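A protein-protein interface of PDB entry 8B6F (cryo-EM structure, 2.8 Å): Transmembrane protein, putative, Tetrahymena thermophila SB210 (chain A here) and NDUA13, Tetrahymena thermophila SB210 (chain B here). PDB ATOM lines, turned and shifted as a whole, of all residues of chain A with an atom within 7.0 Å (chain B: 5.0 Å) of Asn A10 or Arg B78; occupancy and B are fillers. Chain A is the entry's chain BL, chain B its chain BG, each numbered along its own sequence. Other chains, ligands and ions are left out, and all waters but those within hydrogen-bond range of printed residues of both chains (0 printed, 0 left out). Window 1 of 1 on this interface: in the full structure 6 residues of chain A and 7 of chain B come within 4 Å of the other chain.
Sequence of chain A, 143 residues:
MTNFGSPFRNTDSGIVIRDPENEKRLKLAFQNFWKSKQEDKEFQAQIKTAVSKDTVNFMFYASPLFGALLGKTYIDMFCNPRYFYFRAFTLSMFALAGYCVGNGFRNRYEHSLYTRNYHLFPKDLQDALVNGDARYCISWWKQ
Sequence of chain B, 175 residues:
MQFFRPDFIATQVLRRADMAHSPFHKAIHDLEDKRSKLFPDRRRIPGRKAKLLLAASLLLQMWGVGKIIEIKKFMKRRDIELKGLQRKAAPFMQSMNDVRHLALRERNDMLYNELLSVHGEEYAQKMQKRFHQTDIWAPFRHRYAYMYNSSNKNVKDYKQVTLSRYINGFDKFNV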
ATOM      1  N   PHE A   4     -17.723   3.514  -3.222  1.00  0.00           N
ATOM      2  CA  PHE A   4     -16.329   3.129  -3.382  1.00  0.00           C
ATOM      3  C   PHE A   4     -15.340   4.107  -2.772  1.00  0.00           C
ATOM      4  O   PHE A   4     -14.202   3.714  -2.499  1.00  0.00           O
ATOM      5  CB  PHE A   4     -15.992   2.966  -4.872  1.00  0.00           C
ATOM      6  CG  PHE A   4     -16.855   1.966  -5.583  1.00  0.00           C
ATOM      7  CD1 PHE A   4     -16.524   0.621  -5.584  1.00  0.00           C
ATOM      8  CD2 PHE A   4     -17.997   2.369  -6.251  1.00  0.00           C
ATOM      9  CE1 PHE A   4     -17.316  -0.302  -6.236  1.00  0.00           C
ATOM     10  CE2 PHE A   4     -18.793   1.450  -6.906  1.00  0.00           C
ATOM     11  CZ  PHE A   4     -18.451   0.113  -6.898  1.00  0.00           C
ATOM     12  N   GLY A   5     -15.733   5.353  -2.544  1.00  0.00           N
ATOM     13  CA  GLY A   5     -14.790   6.332  -2.057  1.00  0.00           C
ATOM     14  C   GLY A   5     -13.852   6.779  -3.165  1.00  0.00           C
ATOM     15  O   GLY A   5     -14.079   6.556  -4.353  1.00  0.00           O
ATOM     16  N   SER A   6     -12.777   7.430  -2.747  1.00  0.00           N
ATOM     17  CA  SER A   6     -11.802   7.923  -3.703  1.00  0.00           C
ATOM     18  C   SER A   6     -11.096   6.748  -4.376  1.00  0.00           C
ATOM     19  O   SER A   6     -10.827   5.732  -3.730  1.00  0.00           O
ATOM     20  CB  SER A   6     -10.784   8.827  -3.015  1.00  0.00           C
ATOM     21  OG  SER A   6     -10.111   8.133  -1.983  1.00  0.00           O
ATOM     22  N   PRO A   7     -10.783   6.854  -5.672  1.00  0.00           N
ATOM     23  CA  PRO A   7     -10.074   5.756  -6.341  1.00  0.00           C
ATOM     24  C   PRO A   7      -8.592   5.700  -6.025  1.00  0.00           C
ATOM     25  O   PRO A   7      -7.979   4.641  -6.211  1.00  0.00           O
ATOM     26  CB  PRO A   7     -10.304   6.053  -7.828  1.00  0.00           C
ATOM     27  CG  PRO A   7     -10.410   7.532  -7.881  1.00  0.00           C
ATOM     28  CD  PRO A   7     -11.086   7.956  -6.602  1.00  0.00           C
ATOM     29  N   PHE A   8      -7.998   6.799  -5.563  1.00  0.00           N
ATOM     30  CA  PHE A   8      -6.559   6.827  -5.330  1.00  0.00           C
ATOM     31  C   PHE A   8      -6.178   6.097  -4.048  1.00  0.00           C
ATOM     32  O   PHE A   8      -5.129   5.448  -3.993  1.00  0.00           O
ATOM     33  CB  PHE A   8      -6.072   8.274  -5.281  1.00  0.00           C
ATOM     34  CG  PHE A   8      -6.574   9.117  -6.415  1.00  0.00           C
ATOM     35  CD1 PHE A   8      -5.983   9.047  -7.662  1.00  0.00           C
ATOM     36  CD2 PHE A   8      -7.638   9.984  -6.229  1.00  0.00           C
ATOM     37  CE1 PHE A   8      -6.444   9.821  -8.707  1.00  0.00           C
ATOM     38  CE2 PHE A   8      -8.103  10.761  -7.269  1.00  0.00           C
ATOM     39  CZ  PHE A   8      -7.505  10.679  -8.510  1.00  0.00           C
ATOM     40  N   ARG A   9      -7.008   6.191  -3.013  1.00  0.00           N
ATOM     41  CA  ARG A   9      -6.698   5.625  -1.709  1.00  0.00           C
ATOM     42  C   ARG A   9      -7.926   4.911  -1.166  1.00  0.00           C
ATOM     43  O   ARG A   9      -9.043   5.084  -1.657  1.00  0.00           O
ATOM     44  CB  ARG A   9      -6.230   6.707  -0.731  1.00  0.00           C
ATOM     45  CG  ARG A   9      -7.282   7.754  -0.452  1.00  0.00           C
ATOM     46  CD  ARG A   9      -6.692   8.985   0.202  1.00  0.00           C
ATOM     47  NE  ARG A   9      -7.707  10.011   0.397  1.00  0.00           N
ATOM     48  CZ  ARG A   9      -8.157  10.813  -0.558  1.00  0.00           C
ATOM     49  NH1 ARG A   9      -7.705  10.733  -1.799  1.00  0.00           N
ATOM     50  NH2 ARG A   9      -9.088  11.716  -0.263  1.00  0.00           N
ATOM     51  N   ASN A  10      -7.705   4.094  -0.140  1.00  0.00           N
ATOM     52  CA  ASN A  10      -8.779   3.364   0.530  1.00  0.00           C
ATOM     53  C   ASN A  10      -9.381   4.285   1.584  1.00  0.00           C
ATOM     54  O   ASN A  10      -8.878   4.380   2.705  1.00  0.00           O
ATOM     55  CB  ASN A  10      -8.243   2.075   1.143  1.00  0.00           C
ATOM     56  CG  ASN A  10      -9.343   1.108   1.524  1.00  0.00           C
ATOM     57  OD1 ASN A  10     -10.475   1.510   1.785  1.00  0.00           O
ATOM     58  ND2 ASN A  10      -9.013  -0.175   1.560  1.00  0.00           N
ATOM     59  N   THR A  11     -10.464   4.968   1.223  1.00  0.00           N
ATOM     60  CA  THR A  11     -11.052   5.968   2.103  1.00  0.00           C
ATOM     61  C   THR A  11     -11.603   5.327   3.372  1.00  0.00           C
ATOM     62  O   THR A  11     -12.219   4.259   3.333  1.00  0.00           O
ATOM     63  CB  THR A  11     -12.164   6.726   1.375  1.00  0.00           C
ATOM     64  OG1 THR A  11     -11.604   7.474   0.288  1.00  0.00           O
ATOM     65  CG2 THR A  11     -12.886   7.685   2.316  1.00  0.00           C
ATOM     66  N   ASP A  12     -11.384   6.001   4.502  1.00  0.00           N
ATOM     67  CA  ASP A  12     -11.893   5.556   5.800  1.00  0.00           C
ATOM     68  C   ASP A  12     -11.440   4.135   6.117  1.00  0.00           C
ATOM     69  O   ASP A  12     -12.190   3.336   6.682  1.00  0.00           O
ATOM     70  CB  ASP A  12     -13.417   5.662   5.857  1.00  0.00           C
ATOM     71  CG  ASP A  12     -13.907   7.093   5.765  1.00  0.00           C
ATOM     72  OD1 ASP A  12     -13.163   8.004   6.185  1.00  0.00           O
ATOM     73  OD2 ASP A  12     -15.035   7.307   5.275  1.00  0.00           O
ATOM     74  N   SER A  13     -10.200   3.817   5.762  1.00  0.00           N
ATOM     75  CA  SER A  13      -9.609   2.517   6.046  1.00  0.00           C
ATOM     76  C   SER A  13      -8.633   2.676   7.204  1.00  0.00           C
ATOM     77  O   SER A  13      -7.695   3.475   7.123  1.00  0.00           O
ATOM     78  CB  SER A  13      -8.901   1.959   4.812  1.00  0.00           C
ATOM     79  OG  SER A  13      -8.427   0.645   5.047  1.00  0.00           O
ATOM     80  N   GLY A  14      -8.853   1.917   8.272  1.00  0.00           N
ATOM     81  CA  GLY A  14      -8.051   2.081   9.465  1.00  0.00           C
ATOM     82  C   GLY A  14      -8.638   3.135  10.376  1.00  0.00           C
ATOM     83  O   GLY A  14      -9.549   2.856  11.160  1.00  0.00           O
ATOM     84  N   ILE A  15      -8.117   4.353  10.284  1.00  0.00           N
ATOM     85  CA  ILE A  15      -8.619   5.495  11.038  1.00  0.00           C
ATOM     86  C   ILE A  15      -9.576   6.280  10.154  1.00  0.00           C
ATOM     87  O   ILE A  15      -9.321   6.473   8.959  1.00  0.00           O
ATOM     88  CB  ILE A  15      -7.460   6.384  11.532  1.00  0.00           C
ATOM     89  CG1 ILE A  15      -7.989   7.450  12.495  1.00  0.00           C
ATOM     90  CG2 ILE A  15      -6.736   7.028  10.352  1.00  0.00           C
ATOM     91  CD1 ILE A  15      -6.914   8.323  13.109  1.00  0.00           C
ATOM     92  N   PHE B  74     -12.935  -2.788  -9.583  1.00  0.00           N
ATOM     93  CA  PHE B  74     -12.372  -1.738  -8.740  1.00  0.00           C
ATOM     94  C   PHE B  74     -11.305  -2.301  -7.813  1.00  0.00           C
ATOM     95  O   PHE B  74     -10.248  -1.689  -7.623  1.00  0.00           O
ATOM     96  CB  PHE B  74     -13.485  -1.063  -7.937  1.00  0.00           C
ATOM     97  CG  PHE B  74     -13.015   0.091  -7.102  1.00  0.00           C
ATOM     98  CD1 PHE B  74     -12.808   1.336  -7.672  1.00  0.00           C
ATOM     99  CD2 PHE B  74     -12.796  -0.064  -5.743  1.00  0.00           C
ATOM    100  CE1 PHE B  74     -12.382   2.404  -6.903  1.00  0.00           C
ATOM    101  CE2 PHE B  74     -12.370   0.999  -4.970  1.00  0.00           C
ATOM    102  CZ  PHE B  74     -12.163   2.234  -5.550  1.00  0.00           C
ATOM    103  N   MET B  75     -11.564  -3.469  -7.224  1.00  0.00           N
ATOM    104  CA  MET B  75     -10.559  -4.117  -6.389  1.00  0.00           C
ATOM    105  C   MET B  75      -9.292  -4.400  -7.184  1.00  0.00           C
ATOM    106  O   MET B  75      -8.179  -4.194  -6.690  1.00  0.00           O
ATOM    107  CB  MET B  75     -11.121  -5.412  -5.805  1.00  0.00           C
ATOM    108  CG  MET B  75     -12.201  -5.205  -4.759  1.00  0.00           C
ATOM    109  SD  MET B  75     -12.918  -6.765  -4.210  1.00  0.00           S
ATOM    110  CE  MET B  75     -13.979  -6.210  -2.883  1.00  0.00           C
ATOM    111  N   LYS B  76      -9.445  -4.860  -8.427  1.00  0.00           N
ATOM    112  CA  LYS B  76      -8.291  -5.123  -9.279  1.00  0.00           C
ATOM    113  C   LYS B  76      -7.548  -3.837  -9.613  1.00  0.00           C
ATOM    114  O   LYS B  76      -6.313  -3.825  -9.673  1.00  0.00           O
ATOM    115  CB  LYS B  76      -8.739  -5.837 -10.555  1.00  0.00           C
ATOM    116  CG  LYS B  76      -7.592  -6.301 -11.439  1.00  0.00           C
ATOM    117  CD  LYS B  76      -8.091  -7.041 -12.672  1.00  0.00           C
ATOM    118  CE  LYS B  76      -8.722  -8.378 -12.310  1.00  0.00           C
ATOM    119  NZ  LYS B  76      -9.103  -9.158 -13.521  1.00  0.00           N
ATOM    120  N   ARG B  77      -8.279  -2.748  -9.850  1.00  0.00           N
ATOM    121  CA  ARG B  77      -7.631  -1.461 -10.077  1.00  0.00           C
ATOM    122  C   ARG B  77      -6.729  -1.087  -8.909  1.00  0.00           C
ATOM    123  O   ARG B  77      -5.592  -0.645  -9.107  1.00  0.00           O
ATOM    124  CB  ARG B  77      -8.685  -0.378 -10.308  1.00  0.00           C
ATOM    125  CG  ARG B  77      -9.292  -0.400 -11.701  1.00  0.00           C
ATOM    126  CD  ARG B  77     -10.188   0.804 -11.938  1.00  0.00           C
ATOM    127  NE  ARG B  77     -11.524   0.618 -11.382  1.00  0.00           N
ATOM    128  CZ  ARG B  77     -12.565   0.154 -12.062  1.00  0.00           C
ATOM    129  NH1 ARG B  77     -12.464  -0.194 -13.332  1.00  0.00           N
ATOM    130  NH2 ARG B  77     -13.738   0.037 -11.448  1.00  0.00           N
ATOM    131  N   ARG B  78      -7.214  -1.262  -7.680  1.00  0.00           N
ATOM    132  CA  ARG B  78      -6.388  -0.977  -6.512  1.00  0.00           C
ATOM    133  C   ARG B  78      -5.280  -2.007  -6.349  1.00  0.00           C
ATOM    134  O   ARG B  78      -4.199  -1.679  -5.848  1.00  0.00           O
ATOM    135  CB  ARG B  78      -7.255  -0.910  -5.256  1.00  0.00           C
ATOM    136  CG  ARG B  78      -8.329   0.164  -5.336  1.00  0.00           C
ATOM    137  CD  ARG B  78      -8.891   0.522  -3.973  1.00  0.00           C
ATOM    138  NE  ARG B  78      -9.478  -0.628  -3.297  1.00  0.00           N
ATOM    139  CZ  ARG B  78     -10.155  -0.561  -2.161  1.00  0.00           C
ATOM    140  NH1 ARG B  78     -10.361   0.592  -1.546  1.00  0.00           N
ATOM    141  NH2 ARG B  78     -10.640  -1.677  -1.628  1.00  0.00           N
ATOM    142  N   ASP B  79      -5.522  -3.251  -6.765  1.00  0.00           N
ATOM    143  CA  ASP B  79      -4.476  -4.266  -6.704  1.00  0.00           C
ATOM    144  C   ASP B  79      -3.294  -3.902  -7.589  1.00  0.00           C
ATOM    145  O   ASP B  79      -2.158  -4.293  -7.296  1.00  0.00           O
ATOM    146  CB  ASP B  79      -5.039  -5.622  -7.123  1.00  0.00           C
ATOM    147  CG  ASP B  79      -6.148  -6.100  -6.210  1.00  0.00           C
ATOM    148  OD1 ASP B  79      -6.428  -5.414  -5.204  1.00  0.00           O
ATOM    149  OD2 ASP B  79      -6.746  -7.157  -6.503  1.00  0.00           O
ATOM    150  N   ILE B  80      -3.535  -3.168  -8.674  1.00  0.00           N
ATOM    151  CA  ILE B  80      -2.433  -2.709  -9.516  1.00  0.00           C
ATOM    152  C   ILE B  80      -1.470  -1.857  -8.700  1.00  0.00           C
ATOM    153  O   ILE B  80      -0.251  -2.058  -8.737  1.00  0.00           O
ATOM    154  CB  ILE B  80      -2.973  -1.944 -10.739  1.00  0.00           C
ATOM    155  CG1 ILE B  80      -3.654  -2.914 -11.709  1.00  0.00           C
ATOM    156  CG2 ILE B  80      -1.849  -1.186 -11.445  1.00  0.00           C
ATOM    157  CD1 ILE B  80      -4.385  -2.236 -12.856  1.00  0.00           C
ATOM    158  N   GLU B  81      -2.001  -0.884  -7.956  1.00  0.00           N
ATOM    159  CA  GLU B  81      -1.137  -0.039  -7.139  1.00  0.00           C
ATOM    160  C   GLU B  81      -0.487  -0.829  -6.010  1.00  0.00           C
ATOM    161  O   GLU B  81       0.681  -0.596  -5.680  1.00  0.00           O
ATOM    162  CB  GLU B  81      -1.933   1.137  -6.576  1.00  0.00           C
ATOM    163  CG  GLU B  81      -2.210   2.231  -7.588  1.00  0.00           C
ATOM    164  CD  GLU B  81      -2.606   3.536  -6.931  1.00  0.00           C
ATOM    165  OE1 GLU B  81      -2.956   3.516  -5.734  1.00  0.00           O
ATOM    166  OE2 GLU B  81      -2.558   4.584  -7.608  1.00  0.00           O
ATOM    167  N   LEU B  82      -1.222  -1.761  -5.400  1.00  0.00           N
ATOM    168  CA  LEU B  82      -0.618  -2.589  -4.362  1.00  0.00           C
ATOM    169  C   LEU B  82       0.546  -3.391  -4.924  1.00  0.00           C
ATOM    170  O   LEU B  82       1.596  -3.512  -4.286  1.00  0.00           O
ATOM    171  CB  LEU B  82      -1.657  -3.523  -3.741  1.00  0.00           C
ATOM    172  CG  LEU B  82      -1.121  -4.380  -2.585  1.00  0.00           C
ATOM    173  CD1 LEU B  82      -0.813  -3.556  -1.349  1.00  0.00           C
ATOM    174  CD2 LEU B  82      -2.095  -5.481  -2.247  1.00  0.00           C
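Printed residues of chain B within 4 Å of Phe A4: Phe B74 (3.8 Å).
Of the printed residues of chain B, Phe A8 touches Glu B81 (3.4 Å).
Asn A10 touches just one residue of chain B: Arg B78 (3.3 Å).
Thr A11 touches none of the printed residues of chain B.
Printed residues of chain A within 4 Å of Phe B74: Phe A4 (3.8 Å).
Of the printed residues of chain A, Arg B78 touches Asn A10 (3.3 Å).
Printed residues of chain A within 4 Å of Glu B81: Phe A8.
The nearest printed residue of chain B that does not touch Asn A10 is Phe B74 (7.0 Å).
The nearest printed residue of chain B that does not touch Phe A8 is Phe B74 (6.2 Å).
Among the printed residues, merely in contact across the chains: Phe A4 with Phe B74 (3.8 Å).
The backbone carbonyl oxygen of Phe A8 lies close to the side-chain carboxylate of Glu B81 (3.4 Å).
The side-chain amide oxygen (OD1) of Asn A10 lies close to the guanidinium group (NH1) of Arg B78.
Of the 12 printed residues of chain A, 3 touch a printed residue of chain B.
Of the 9 printed residues of chain B, 3 touch a printed residue of chain A.
Printed residues of chain B that touch a printed residue of chain A: Phe B74, Arg B78 and Glu B81.
Among the printed residues, no Asp or Glu carboxylate lies within 4 Å of a Lys or Arg side-chain nitrogen of the other chain.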
